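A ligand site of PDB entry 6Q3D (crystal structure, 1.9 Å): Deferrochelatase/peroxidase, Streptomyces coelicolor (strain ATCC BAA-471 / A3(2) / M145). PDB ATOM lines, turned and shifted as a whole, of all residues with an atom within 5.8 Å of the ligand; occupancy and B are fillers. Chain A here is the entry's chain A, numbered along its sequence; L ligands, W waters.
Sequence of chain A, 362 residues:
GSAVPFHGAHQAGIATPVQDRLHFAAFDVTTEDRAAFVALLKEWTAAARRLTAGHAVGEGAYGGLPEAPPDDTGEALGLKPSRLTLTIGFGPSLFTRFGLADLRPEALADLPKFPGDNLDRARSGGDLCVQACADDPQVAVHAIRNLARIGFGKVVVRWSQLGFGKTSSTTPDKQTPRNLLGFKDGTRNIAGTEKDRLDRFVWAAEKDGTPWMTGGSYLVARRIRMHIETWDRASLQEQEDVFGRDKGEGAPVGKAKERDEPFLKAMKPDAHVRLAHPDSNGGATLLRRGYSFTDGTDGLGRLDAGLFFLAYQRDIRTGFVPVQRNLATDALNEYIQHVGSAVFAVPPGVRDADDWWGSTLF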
ATOM      1  N   ASN A 179      -2.271   9.603   8.985  1.00  0.00           N
ATOM      2  CA  ASN A 179      -2.568  10.366  10.176  1.00  0.00           C
ATOM      3  C   ASN A 179      -1.758   9.823  11.345  1.00  0.00           C
ATOM      4  O   ASN A 179      -0.996   8.859  11.212  1.00  0.00           O
ATOM      5  CB  ASN A 179      -4.061  10.346  10.476  1.00  0.00           C
ATOM      6  CG  ASN A 179      -4.643   8.944  10.499  1.00  0.00           C
ATOM      7  OD1 ASN A 179      -4.104   8.023  11.134  1.00  0.00           O
ATOM      8  ND2 ASN A 179      -5.796   8.785   9.850  1.00  0.00           N
ATOM      9  N   LEU A 181      -2.614   8.143  13.785  1.00  0.00           N
ATOM     10  CA  LEU A 181      -2.962   6.780  14.134  1.00  0.00           C
ATOM     11  C   LEU A 181      -2.263   5.730  13.276  1.00  0.00           C
ATOM     12  O   LEU A 181      -2.480   4.537  13.515  1.00  0.00           O
ATOM     13  CB  LEU A 181      -4.472   6.565  13.998  1.00  0.00           C
ATOM     14  CG  LEU A 181      -5.369   7.464  14.827  1.00  0.00           C
ATOM     15  CD1 LEU A 181      -6.812   7.001  14.636  1.00  0.00           C
ATOM     16  CD2 LEU A 181      -4.952   7.376  16.303  1.00  0.00           C
ATOM     17  N   PHE A 183      -2.647   5.260   9.832  1.00  0.00           N
ATOM     18  CA  PHE A 183      -3.322   4.800   8.633  1.00  0.00           C
ATOM     19  C   PHE A 183      -3.224   5.834   7.523  1.00  0.00           C
ATOM     20  O   PHE A 183      -3.198   7.050   7.780  1.00  0.00           O
ATOM     21  CB  PHE A 183      -4.795   4.468   8.912  1.00  0.00           C
ATOM     22  CG  PHE A 183      -5.019   3.129   9.592  1.00  0.00           C
ATOM     23  CD1 PHE A 183      -4.739   2.941  10.949  1.00  0.00           C
ATOM     24  CD2 PHE A 183      -5.536   2.064   8.872  1.00  0.00           C
ATOM     25  CE1 PHE A 183      -4.961   1.709  11.553  1.00  0.00           C
ATOM     26  CE2 PHE A 183      -5.748   0.830   9.490  1.00  0.00           C
ATOM     27  CZ  PHE A 183      -5.459   0.652  10.826  1.00  0.00           C
ATOM     28  N   LYS A 184      -3.124   5.359   6.271  1.00  0.00           N
ATOM     29  CA  LYS A 184      -3.268   6.253   5.131  1.00  0.00           C
ATOM     30  C   LYS A 184      -4.614   6.962   5.234  1.00  0.00           C
ATOM     31  O   LYS A 184      -5.602   6.376   5.671  1.00  0.00           O
ATOM     32  CB  LYS A 184      -3.161   5.477   3.810  1.00  0.00           C
ATOM     33  CG  LYS A 184      -1.865   4.661   3.696  1.00  0.00           C
ATOM     34  CD  LYS A 184      -1.936   3.646   2.540  1.00  0.00           C
ATOM     35  CE  LYS A 184      -0.641   3.625   1.713  1.00  0.00           C
ATOM     36  NZ  LYS A 184      -0.555   2.403   0.833  1.00  0.00           N
ATOM     37  N   ASP A 185      -4.642   8.243   4.893  1.00  0.00           N
ATOM     38  CA  ASP A 185      -5.837   9.073   5.083  1.00  0.00           C
ATOM     39  C   ASP A 185      -6.058   9.871   3.807  1.00  0.00           C
ATOM     40  O   ASP A 185      -5.243  10.729   3.488  1.00  0.00           O
ATOM     41  CB  ASP A 185      -5.674  10.005   6.301  1.00  0.00           C
ATOM     42  CG  ASP A 185      -7.023  10.387   6.971  1.00  0.00           C
ATOM     43  OD1 ASP A 185      -8.017  10.665   6.267  1.00  0.00           O
ATOM     44  OD2 ASP A 185      -7.074  10.426   8.216  1.00  0.00           O
ATOM     45  N   GLY A 186      -7.150   9.606   3.102  1.00  0.00           N
ATOM     46  CA  GLY A 186      -7.495  10.359   1.900  1.00  0.00           C
ATOM     47  C   GLY A 186      -7.667   9.526   0.636  1.00  0.00           C
ATOM     48  O   GLY A 186      -7.907  10.108  -0.439  1.00  0.00           O
ATOM     49  N   THR A 187      -7.579   8.198   0.718  1.00  0.00           N
ATOM     50  CA  THR A 187      -7.675   7.337  -0.446  1.00  0.00           C
ATOM     51  C   THR A 187      -8.931   7.638  -1.264  1.00  0.00           C
ATOM     52  O   THR A 187      -8.852   7.907  -2.474  1.00  0.00           O
ATOM     53  CB  THR A 187      -7.653   5.875   0.007  1.00  0.00           C
ATOM     54  OG1 THR A 187      -6.479   5.672   0.793  1.00  0.00           O
ATOM     55  CG2 THR A 187      -7.668   4.908  -1.177  1.00  0.00           C
ATOM     56  N   ARG A 188     -10.094   7.596  -0.622  1.00  0.00           N
ATOM     57  CA  ARG A 188     -11.377   7.767  -1.324  1.00  0.00           C
ATOM     58  C   ARG A 188     -11.953   9.130  -0.968  1.00  0.00           C
ATOM     59  O   ARG A 188     -12.956   9.255  -0.258  1.00  0.00           O
ATOM     60  CB  ARG A 188     -12.343   6.614  -0.978  1.00  0.00           C
ATOM     61  CG  ARG A 188     -12.023   5.339  -1.746  1.00  0.00           C
ATOM     62  CD  ARG A 188     -13.156   4.322  -1.620  1.00  0.00           C
ATOM     63  NE  ARG A 188     -14.412   4.989  -1.348  1.00  0.00           N
ATOM     64  CZ  ARG A 188     -15.271   5.396  -2.278  1.00  0.00           C
ATOM     65  NH1 ARG A 188     -16.388   6.015  -1.927  1.00  0.00           N
ATOM     66  NH2 ARG A 188     -15.006   5.175  -3.565  1.00  0.00           N
ATOM     67  N   ASN A 189     -11.285  10.166  -1.490  1.00  0.00           N
ATOM     68  CA  ASN A 189     -11.641  11.566  -1.381  1.00  0.00           C
ATOM     69  C   ASN A 189     -12.117  12.049  -2.747  1.00  0.00           C
ATOM     70  O   ASN A 189     -12.206  11.270  -3.696  1.00  0.00           O
ATOM     71  CB  ASN A 189     -10.444  12.359  -0.861  1.00  0.00           C
ATOM     72  CG  ASN A 189     -10.836  13.670  -0.278  1.00  0.00           C
ATOM     73  OD1 ASN A 189     -11.928  13.812   0.289  1.00  0.00           O
ATOM     74  ND2 ASN A 189      -9.927  14.657  -0.359  1.00  0.00           N
ATOM     75  N   ILE A 224     -10.254  17.655  16.559  1.00  0.00           N
ATOM     76  CA  ILE A 224     -10.514  16.297  17.044  1.00  0.00           C
ATOM     77  C   ILE A 224      -9.287  15.791  17.784  1.00  0.00           C
ATOM     78  O   ILE A 224      -8.246  15.514  17.160  1.00  0.00           O
ATOM     79  CB  ILE A 224     -10.902  15.348  15.909  1.00  0.00           C
ATOM     80  CG1 ILE A 224     -12.115  15.908  15.162  1.00  0.00           C
ATOM     81  CG2 ILE A 224     -11.159  13.954  16.456  1.00  0.00           C
ATOM     82  CD1 ILE A 224     -12.486  15.099  13.948  1.00  0.00           C
ATOM     83  N   MET A 226      -7.114  12.975  19.693  1.00  0.00           N
ATOM     84  CA  MET A 226      -6.917  11.524  19.598  1.00  0.00           C
ATOM     85  C   MET A 226      -6.375  11.001  20.916  1.00  0.00           C
ATOM     86  O   MET A 226      -5.377  11.524  21.445  1.00  0.00           O
ATOM     87  CB  MET A 226      -5.954  11.183  18.462  1.00  0.00           C
ATOM     88  CG  MET A 226      -6.482  11.502  17.097  1.00  0.00           C
ATOM     89  SD  MET A 226      -5.141  11.346  15.900  1.00  0.00           S
ATOM     90  CE  MET A 226      -6.081  11.555  14.392  1.00  0.00           C
ATOM     91  N   PHE A 243     -11.201   0.497  11.363  1.00  0.00           N
ATOM     92  CA  PHE A 243     -11.306   1.238  10.108  1.00  0.00           C
ATOM     93  C   PHE A 243     -11.969   0.441   8.996  1.00  0.00           C
ATOM     94  O   PHE A 243     -12.778   1.001   8.235  1.00  0.00           O
ATOM     95  CB  PHE A 243      -9.928   1.729   9.686  1.00  0.00           C
ATOM     96  CG  PHE A 243      -9.543   2.974  10.375  1.00  0.00           C
ATOM     97  CD1 PHE A 243     -10.257   4.157  10.134  1.00  0.00           C
ATOM     98  CD2 PHE A 243      -8.550   2.971  11.335  1.00  0.00           C
ATOM     99  CE1 PHE A 243      -9.948   5.316  10.813  1.00  0.00           C
ATOM    100  CE2 PHE A 243      -8.237   4.122  12.016  1.00  0.00           C
ATOM    101  CZ  PHE A 243      -8.935   5.305  11.748  1.00  0.00           C
ATOM    102  N   ARG A 245      -9.803  -1.309   6.946  1.00  0.00           N
ATOM    103  CA  ARG A 245      -8.699  -1.400   6.001  1.00  0.00           C
ATOM    104  C   ARG A 245      -7.492  -1.863   6.790  1.00  0.00           C
ATOM    105  O   ARG A 245      -7.402  -1.645   7.999  1.00  0.00           O
ATOM    106  CB  ARG A 245      -8.420  -0.038   5.330  1.00  0.00           C
ATOM    107  CG  ARG A 245      -9.522   0.556   4.466  1.00  0.00           C
ATOM    108  CD  ARG A 245      -9.019   1.841   3.826  1.00  0.00           C
ATOM    109  NE  ARG A 245      -9.962   2.424   2.878  1.00  0.00           N
ATOM    110  CZ  ARG A 245      -9.842   2.325   1.559  1.00  0.00           C
ATOM    111  NH1 ARG A 245      -8.790   1.690   1.038  1.00  0.00           N
ATOM    112  NH2 ARG A 245     -10.750   2.883   0.752  1.00  0.00           N
ATOM    113  N   PRO A 262     -13.655  -0.812  -1.769  1.00  0.00           N
ATOM    114  CA  PRO A 262     -14.034  -1.532  -0.547  1.00  0.00           C
ATOM    115  C   PRO A 262     -15.327  -2.301  -0.781  1.00  0.00           C
ATOM    116  O   PRO A 262     -16.233  -1.844  -1.470  1.00  0.00           O
ATOM    117  CB  PRO A 262     -14.211  -0.418   0.482  1.00  0.00           C
ATOM    118  CG  PRO A 262     -14.510   0.796  -0.335  1.00  0.00           C
ATOM    119  CD  PRO A 262     -13.757   0.645  -1.609  1.00  0.00           C
ATOM    120  N   HIS A 272     -15.374   2.316  10.514  1.00  0.00           N
ATOM    121  CA  HIS A 272     -15.426   3.720  10.119  1.00  0.00           C
ATOM    122  C   HIS A 272     -15.732   3.897   8.642  1.00  0.00           C
ATOM    123  O   HIS A 272     -16.635   4.668   8.274  1.00  0.00           O
ATOM    124  CB  HIS A 272     -14.078   4.365  10.457  1.00  0.00           C
ATOM    125  CG  HIS A 272     -14.005   5.816  10.157  1.00  0.00           C
ATOM    126  ND1 HIS A 272     -14.653   6.769  10.901  1.00  0.00           N
ATOM    127  CD2 HIS A 272     -13.309   6.492   9.204  1.00  0.00           C
ATOM    128  CE1 HIS A 272     -14.388   7.970  10.409  1.00  0.00           C
ATOM    129  NE2 HIS A 272     -13.573   7.825   9.383  1.00  0.00           N
ATOM    130  N   VAL A 273     -14.984   3.203   7.782  1.00  0.00           N
ATOM    131  CA  VAL A 273     -15.167   3.329   6.336  1.00  0.00           C
ATOM    132  C   VAL A 273     -16.541   2.815   5.931  1.00  0.00           C
ATOM    133  O   VAL A 273     -17.188   3.370   5.033  1.00  0.00           O
ATOM    134  CB  VAL A 273     -14.054   2.583   5.580  1.00  0.00           C
ATOM    135  CG1 VAL A 273     -14.391   2.524   4.104  1.00  0.00           C
ATOM    136  CG2 VAL A 273     -12.717   3.249   5.795  1.00  0.00           C
ATOM    137  N   ALA A 276     -18.931   5.760   7.029  1.00  0.00           N
ATOM    138  CA  ALA A 276     -18.701   7.032   6.355  1.00  0.00           C
ATOM    139  C   ALA A 276     -18.943   6.958   4.854  1.00  0.00           C
ATOM    140  O   ALA A 276     -19.214   7.996   4.240  1.00  0.00           O
ATOM    141  CB  ALA A 276     -17.266   7.493   6.618  1.00  0.00           C
ATOM    142  N   HIS A 277     -18.883   5.760   4.278  1.00  0.00           N
ATOM    143  CA  HIS A 277     -18.931   5.575   2.829  1.00  0.00           C
ATOM    144  C   HIS A 277     -20.214   6.178   2.244  1.00  0.00           C
ATOM    145  O   HIS A 277     -21.285   6.037   2.836  1.00  0.00           O
ATOM    146  CB  HIS A 277     -18.882   4.079   2.516  1.00  0.00           C
ATOM    147  CG  HIS A 277     -18.590   3.768   1.076  1.00  0.00           C
ATOM    148  ND1 HIS A 277     -19.561   3.777   0.100  1.00  0.00           N
ATOM    149  CD2 HIS A 277     -17.434   3.402   0.459  1.00  0.00           C
ATOM    150  CE1 HIS A 277     -19.018   3.448  -1.062  1.00  0.00           C
ATOM    151  NE2 HIS A 277     -17.733   3.215  -0.863  1.00  0.00           N
ATOM    152  N   PRO A 278     -20.145   6.818   1.066  1.00  0.00           N
ATOM    153  CA  PRO A 278     -21.371   7.422   0.495  1.00  0.00           C
ATOM    154  C   PRO A 278     -22.555   6.474   0.392  1.00  0.00           C
ATOM    155  O   PRO A 278     -23.693   6.898   0.643  1.00  0.00           O
ATOM    156  CB  PRO A 278     -20.900   7.892  -0.891  1.00  0.00           C
ATOM    157  CG  PRO A 278     -19.440   8.180  -0.710  1.00  0.00           C
ATOM    158  CD  PRO A 278     -18.943   7.163   0.294  1.00  0.00           C
ATOM    159  N   LEU A 286     -18.078  14.075   0.662  1.00  0.00           N
ATOM    160  CA  LEU A 286     -17.326  15.197   1.197  1.00  0.00           C
ATOM    161  C   LEU A 286     -15.976  15.309   0.514  1.00  0.00           C
ATOM    162  O   LEU A 286     -15.445  14.328   0.010  1.00  0.00           O
ATOM    163  CB  LEU A 286     -17.093  15.037   2.705  1.00  0.00           C
ATOM    164  CG  LEU A 286     -18.354  14.763   3.500  1.00  0.00           C
ATOM    165  CD1 LEU A 286     -18.008  14.188   4.854  1.00  0.00           C
ATOM    166  CD2 LEU A 286     -19.113  16.077   3.652  1.00  0.00           C
ATOM    167  N   ARG A 288     -12.472  16.028   1.890  1.00  0.00           N
ATOM    168  CA  ARG A 288     -11.707  16.150   3.123  1.00  0.00           C
ATOM    169  C   ARG A 288     -10.366  16.826   2.830  1.00  0.00           C
ATOM    170  O   ARG A 288      -9.725  16.560   1.817  1.00  0.00           O
ATOM    171  CB  ARG A 288     -11.503  14.779   3.761  1.00  0.00           C
ATOM    172  CG  ARG A 288     -12.787  14.242   4.439  1.00  0.00           C
ATOM    173  CD  ARG A 288     -12.681  12.767   4.853  1.00  0.00           C
ATOM    174  NE  ARG A 288     -12.520  11.895   3.682  1.00  0.00           N
ATOM    175  CZ  ARG A 288     -11.607  10.932   3.577  1.00  0.00           C
ATOM    176  NH1 ARG A 288     -10.761  10.702   4.581  1.00  0.00           N
ATOM    177  NH2 ARG A 288     -11.540  10.198   2.468  1.00  0.00           N
ATOM    178  N   LEU A 307      -6.404  15.626  15.103  1.00  0.00           N
ATOM    179  CA  LEU A 307      -6.596  15.892  13.688  1.00  0.00           C
ATOM    180  C   LEU A 307      -7.459  17.136  13.585  1.00  0.00           C
ATOM    181  O   LEU A 307      -8.512  17.224  14.206  1.00  0.00           O
ATOM    182  CB  LEU A 307      -7.266  14.708  12.987  1.00  0.00           C
ATOM    183  CG  LEU A 307      -7.385  14.857  11.468  1.00  0.00           C
ATOM    184  CD1 LEU A 307      -6.686  13.704  10.759  1.00  0.00           C
ATOM    185  CD2 LEU A 307      -8.850  14.935  11.099  1.00  0.00           C
ATOM    186  N   PHE A 309      -9.799  18.600  11.435  1.00  0.00           N
ATOM    187  CA  PHE A 309     -10.605  18.086  10.330  1.00  0.00           C
ATOM    188  C   PHE A 309     -11.341  19.207   9.591  1.00  0.00           C
ATOM    189  O   PHE A 309     -12.041  20.021  10.205  1.00  0.00           O
ATOM    190  CB  PHE A 309     -11.612  17.072  10.888  1.00  0.00           C
ATOM    191  CG  PHE A 309     -12.490  16.415   9.839  1.00  0.00           C
ATOM    192  CD1 PHE A 309     -13.661  17.037   9.425  1.00  0.00           C
ATOM    193  CD2 PHE A 309     -12.168  15.169   9.308  1.00  0.00           C
ATOM    194  CE1 PHE A 309     -14.502  16.437   8.468  1.00  0.00           C
ATOM    195  CE2 PHE A 309     -12.977  14.554   8.362  1.00  0.00           C
ATOM    196  CZ  PHE A 309     -14.156  15.190   7.933  1.00  0.00           C
ATOM    197  N   PHE A 320     -21.722  17.075   5.617  1.00  0.00           N
ATOM    198  CA  PHE A 320     -21.167  16.707   6.905  1.00  0.00           C
ATOM    199  C   PHE A 320     -22.237  16.262   7.891  1.00  0.00           C
ATOM    200  O   PHE A 320     -21.968  15.410   8.748  1.00  0.00           O
ATOM    201  CB  PHE A 320     -20.374  17.869   7.484  1.00  0.00           C
ATOM    202  CG  PHE A 320     -19.834  17.606   8.850  1.00  0.00           C
ATOM    203  CD1 PHE A 320     -20.605  17.871   9.967  1.00  0.00           C
ATOM    204  CD2 PHE A 320     -18.556  17.088   9.014  1.00  0.00           C
ATOM    205  CE1 PHE A 320     -20.123  17.602  11.246  1.00  0.00           C
ATOM    206  CE2 PHE A 320     -18.062  16.839  10.292  1.00  0.00           C
ATOM    207  CZ  PHE A 320     -18.849  17.093  11.407  1.00  0.00           C
ATOM    208  N   VAL A 323     -23.380  12.492   7.353  1.00  0.00           N
ATOM    209  CA  VAL A 323     -22.279  11.552   7.543  1.00  0.00           C
ATOM    210  C   VAL A 323     -21.884  11.499   9.016  1.00  0.00           C
ATOM    211  O   VAL A 323     -21.658  10.430   9.583  1.00  0.00           O
ATOM    212  CB  VAL A 323     -21.084  11.895   6.643  1.00  0.00           C
ATOM    213  CG1 VAL A 323     -19.967  10.887   6.853  1.00  0.00           C
ATOM    214  CG2 VAL A 323     -21.492  11.929   5.171  1.00  0.00           C
ATOM    215  N   GLN A 324     -21.776  12.664   9.664  1.00  0.00           N
ATOM    216  CA  GLN A 324     -21.417  12.663  11.074  1.00  0.00           C
ATOM    217  C   GLN A 324     -22.511  12.019  11.918  1.00  0.00           C
ATOM    218  O   GLN A 324     -22.215  11.376  12.936  1.00  0.00           O
ATOM    219  CB  GLN A 324     -21.144  14.109  11.532  1.00  0.00           C
ATOM    220  CG  GLN A 324     -20.850  14.254  13.010  1.00  0.00           C
ATOM    221  CD  GLN A 324     -19.554  13.565  13.438  1.00  0.00           C
ATOM    222  OE1 GLN A 324     -18.598  13.467  12.679  1.00  0.00           O
ATOM    223  NE2 GLN A 324     -19.522  13.114  14.673  1.00  0.00           N
ATOM    224  N   LEU A 327     -22.042   8.399  12.104  1.00  0.00           N
ATOM    225  CA  LEU A 327     -20.879   8.006  12.887  1.00  0.00           C
ATOM    226  C   LEU A 327     -21.199   7.806  14.369  1.00  0.00           C
ATOM    227  O   LEU A 327     -20.293   7.520  15.158  1.00  0.00           O
ATOM    228  CB  LEU A 327     -19.760   9.034  12.714  1.00  0.00           C
ATOM    229  CG  LEU A 327     -19.097   9.142  11.329  1.00  0.00           C
ATOM    230  CD1 LEU A 327     -17.753   9.900  11.388  1.00  0.00           C
ATOM    231  CD2 LEU A 327     -18.898   7.767  10.711  1.00  0.00           C
ATOM    232  N   LEU A 332     -14.546   4.088  15.863  1.00  0.00           N
ATOM    233  CA  LEU A 332     -13.496   5.055  16.097  1.00  0.00           C
ATOM    234  C   LEU A 332     -13.806   5.975  17.272  1.00  0.00           C
ATOM    235  O   LEU A 332     -12.882   6.528  17.871  1.00  0.00           O
ATOM    236  CB  LEU A 332     -13.260   5.880  14.826  1.00  0.00           C
ATOM    237  CG  LEU A 332     -12.108   6.881  14.825  1.00  0.00           C
ATOM    238  CD1 LEU A 332     -10.772   6.203  15.155  1.00  0.00           C
ATOM    239  CD2 LEU A 332     -12.035   7.615  13.501  1.00  0.00           C
ATOM    240  N   ILE A 336     -11.377   8.996  19.874  1.00  0.00           N
ATOM    241  CA  ILE A 336     -11.317  10.392  19.477  1.00  0.00           C
ATOM    242  C   ILE A 336     -12.314  11.206  20.300  1.00  0.00           C
ATOM    243  O   ILE A 336     -13.259  10.674  20.884  1.00  0.00           O
ATOM    244  CB  ILE A 336     -11.633  10.589  17.972  1.00  0.00           C
ATOM    245  CG1 ILE A 336     -13.031  10.062  17.637  1.00  0.00           C
ATOM    246  CG2 ILE A 336     -10.587   9.933  17.105  1.00  0.00           C
ATOM    247  CD1 ILE A 336     -13.516  10.553  16.309  1.00  0.00           C
ATOM    248  N   HIS A 338     -14.312  15.148  19.686  1.00  0.00           N
ATOM    249  CA  HIS A 338     -14.438  16.453  19.041  1.00  0.00           C
ATOM    250  C   HIS A 338     -14.416  17.546  20.093  1.00  0.00           C
ATOM    251  O   HIS A 338     -15.284  17.573  20.985  1.00  0.00           O
ATOM    252  CB  HIS A 338     -15.732  16.529  18.231  1.00  0.00           C
ATOM    253  CG  HIS A 338     -15.772  15.575  17.090  1.00  0.00           C
ATOM    254  ND1 HIS A 338     -15.823  15.996  15.772  1.00  0.00           N
ATOM    255  CD2 HIS A 338     -15.773  14.223  17.050  1.00  0.00           C
ATOM    256  CE1 HIS A 338     -15.848  14.935  14.975  1.00  0.00           C
ATOM    257  NE2 HIS A 338     -15.825  13.851  15.726  1.00  0.00           N
HETATM  258  C1  LIG L   1     -12.191   7.590   5.397  1.00  0.00           C
HETATM  259  C2  LIG L   1      -9.505   8.321   9.358  1.00  0.00           C
HETATM  260  C3  LIG L   1     -12.825  11.433  10.932  1.00  0.00           C
HETATM  261  C4  LIG L   1     -15.434  10.856   6.904  1.00  0.00           C
HETATM  262  C5  LIG L   1     -11.203   7.484   6.346  1.00  0.00           C
HETATM  263  C6  LIG L   1     -10.088   6.565   6.304  1.00  0.00           C
HETATM  264  C7  LIG L   1      -9.363   6.758   7.395  1.00  0.00           C
HETATM  265  C8  LIG L   1      -9.974   7.816   8.168  1.00  0.00           C
HETATM  266  C9  LIG L   1      -8.085   6.009   7.790  1.00  0.00           C
HETATM  267  C10 LIG L   1      -9.828   5.526   5.185  1.00  0.00           C
HETATM  268  C11 LIG L   1      -8.997   6.119   4.021  1.00  0.00           C
HETATM  269  C12 LIG L   1      -9.682   7.147   3.147  1.00  0.00           C
HETATM  270  O1  LIG L   1     -10.381   6.717   2.198  1.00  0.00           O
HETATM  271  O2  LIG L   1      -9.512   8.390   3.349  1.00  0.00           O
HETATM  272  C13 LIG L   1     -10.154   9.254  10.117  1.00  0.00           C
HETATM  273  C14 LIG L   1      -9.714   9.789  11.398  1.00  0.00           C
HETATM  274  C15 LIG L   1     -10.648  10.652  11.826  1.00  0.00           C
HETATM  275  C16 LIG L   1     -11.688  10.677  10.839  1.00  0.00           C
HETATM  276  C17 LIG L   1      -8.390   9.404  12.083  1.00  0.00           C
HETATM  277  C18 LIG L   1     -10.661  11.510  13.121  1.00  0.00           C
HETATM  278  C19 LIG L   1      -9.578  11.604  13.903  1.00  0.00           C
HETATM  279  C20 LIG L   1     -13.794  11.547   9.975  1.00  0.00           C
HETATM  280  C21 LIG L   1     -14.920  12.422  10.045  1.00  0.00           C
HETATM  281  C22 LIG L   1     -15.636  12.280   8.914  1.00  0.00           C
HETATM  282  C23 LIG L   1     -14.991  11.285   8.125  1.00  0.00           C
HETATM  283  C24 LIG L   1     -15.147  13.379  11.223  1.00  0.00           C
HETATM  284  C25 LIG L   1     -16.940  12.968   8.463  1.00  0.00           C
HETATM  285  C26 LIG L   1     -17.620  13.765   9.296  1.00  0.00           C
HETATM  286  C27 LIG L   1     -14.756   9.957   6.124  1.00  0.00           C
HETATM  287  C28 LIG L   1     -15.099   9.600   4.776  1.00  0.00           C
HETATM  288  C29 LIG L   1     -14.210   8.697   4.345  1.00  0.00           C
HETATM  289  C30 LIG L   1     -13.268   8.452   5.419  1.00  0.00           C
HETATM  290  C31 LIG L   1     -16.301  10.171   3.975  1.00  0.00           C
HETATM  291  C32 LIG L   1     -14.218   8.044   2.947  1.00  0.00           C
HETATM  292  C33 LIG L   1     -14.909   6.689   3.037  1.00  0.00           C
HETATM  293  C34 LIG L   1     -15.203   6.125   1.673  1.00  0.00           C
HETATM  294  O3  LIG L   1     -14.579   5.099   1.329  1.00  0.00           O
HETATM  295  O4  LIG L   1     -16.044   6.713   0.939  1.00  0.00           O
HETATM  296  N1  LIG L   1     -11.099   8.239   7.505  1.00  0.00           N
HETATM  297  N2  LIG L   1     -11.361   9.818   9.802  1.00  0.00           N
HETATM  298  N3  LIG L   1     -13.866  10.862   8.789  1.00  0.00           N
HETATM  299  N4  LIG L   1     -13.642   9.247   6.489  1.00  0.00           N
HETATM  300 FE1  LIG L   1     -12.592   9.445   8.232  1.00  0.00          FE
HETATM  301  O   HOH W   1     -15.768   9.325  -0.524  1.00  0.00           O
HETATM  302  O   HOH W   2     -10.462  11.619   7.357  1.00  0.00           O
HETATM  303  O   HOH W   3     -11.990   4.528   2.238  1.00  0.00           O
HETATM  304  O   HOH W   4     -17.267  11.302   1.087  1.00  0.00           O
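Water W3 bridges NH2 of Arg 245 (2.5 Å) and O1 of the ligand (2.7 Å). Water W1 bridges the backbone carbonyl oxygen (O) of Arg 188 (2.8 Å) and an oxygen (O4) of the ligand (3.0 Å). Water W2 bridges the side-chain carboxylate (OD1) of Asp 185 (2.8 Å) and the guanidinium group (NH1) of Arg 288 (2.9 Å).
O of Phe 243 lies within hydrogen-bond range of N of Val 273, 3.1 Å away. N of Arg 288 sits at hydrogen-bond distance from OD1 of Asn 189. N of Leu 307 sits at hydrogen-bond distance from O of Ile 224. The side-chain carboxylate (OD2) of Asp 185 is in hydrogen-bond range of the side-chain amide nitrogen (ND2) of Asn 179 (2.6 Å). A ring nitrogen (NE2) of His 277 lies within hydrogen-bond range of the guanidinium group (NH1) of Arg 188, 3.3 Å away. The side-chain amide oxygen (OD1) of Asn 179 sits at hydrogen-bond distance from the backbone NH (N) of Leu 181, 3.0 Å away. NH1 of Arg 288 lies within salt-bridge range of OD1 of Asp 185 (3.2 Å). O of Arg 188 is in hydrogen-bond range of NH2 of Arg 288 (3.2 Å).
Asn 179 touches the ligand (ND2 to C17, 3.5 Å). Leu 181 touches the ligand (CD1 to C17, 3.8 Å). Phe 183 touches the ligand (CB to C9, 3.8 Å). Lys 184 touches the ligand. Asp 185 touches the ligand (OD2 to C2, 3.4 Å). CG2 of Ile 224 touches C19 of the ligand (3.8 Å). Met 226 touches the ligand (CE to C19, 3.5 Å). Phe 243 touches the ligand. NE of Arg 245 touches C10 of the ligand, 3.9 Å away. CG2 of Val 273 touches C10 of the ligand (3.7 Å). CB of Ala 276 touches C28 of the ligand, 3.5 Å away. His 277 touches the ligand (CD2 to O3, 3.4 Å). CD of Pro 278 touches O4 of the ligand, at 3.0 Å. CD1 of Leu 286 touches C25 of the ligand, 3.96 Å away. Leu 307 touches the ligand (CB to C19, 3.98 Å). CE2 of Phe 309 touches C21 of the ligand (3.3 Å). Phe 320 touches the ligand (CE2 to C26, 3.3 Å). OE1 of Gln 324 touches C26 of the ligand (3.5 Å). CD2 of Leu 332 touches C15 of the ligand, at 3.7 Å. Ile 336 touches the ligand (CG2 to C19, 3.8 Å). 25 residues have an atom within 4 Å of the ligand: Asn 179, Leu 181, Phe 183, Lys 184, Asp 185, Gly 186, Thr 187, Arg 188, Ile 224, Met 226, Phe 243, Arg 245, His 272, Val 273, Ala 276, His 277, Pro 278, Leu 286, Arg 288, Leu 307, Phe 309, Phe 320, Gln 324, Leu 332 and Ile 336. The nearest printed residue that does not touch the ligand is Val 323 (4.01 Å).
O2 of the ligand is in hydrogen-bond range of N of Thr 187, at 3.3 Å. A ring nitrogen (NE2) of His 272 binds an iron atom (FE1) of the ligand, at 2.2 Å. NE of Arg 188 lies within salt-bridge range of O3 of the ligand (2.7 Å). NH2 of Arg 288 lies within salt-bridge range of O2 of the ligand (2.9 Å). N of Gly 186 is in hydrogen-bond range of O2 of the ligand (2.7 Å). The backbone NH (N) of Arg 188 sits at hydrogen-bond distance from an oxygen (O1) of the ligand.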
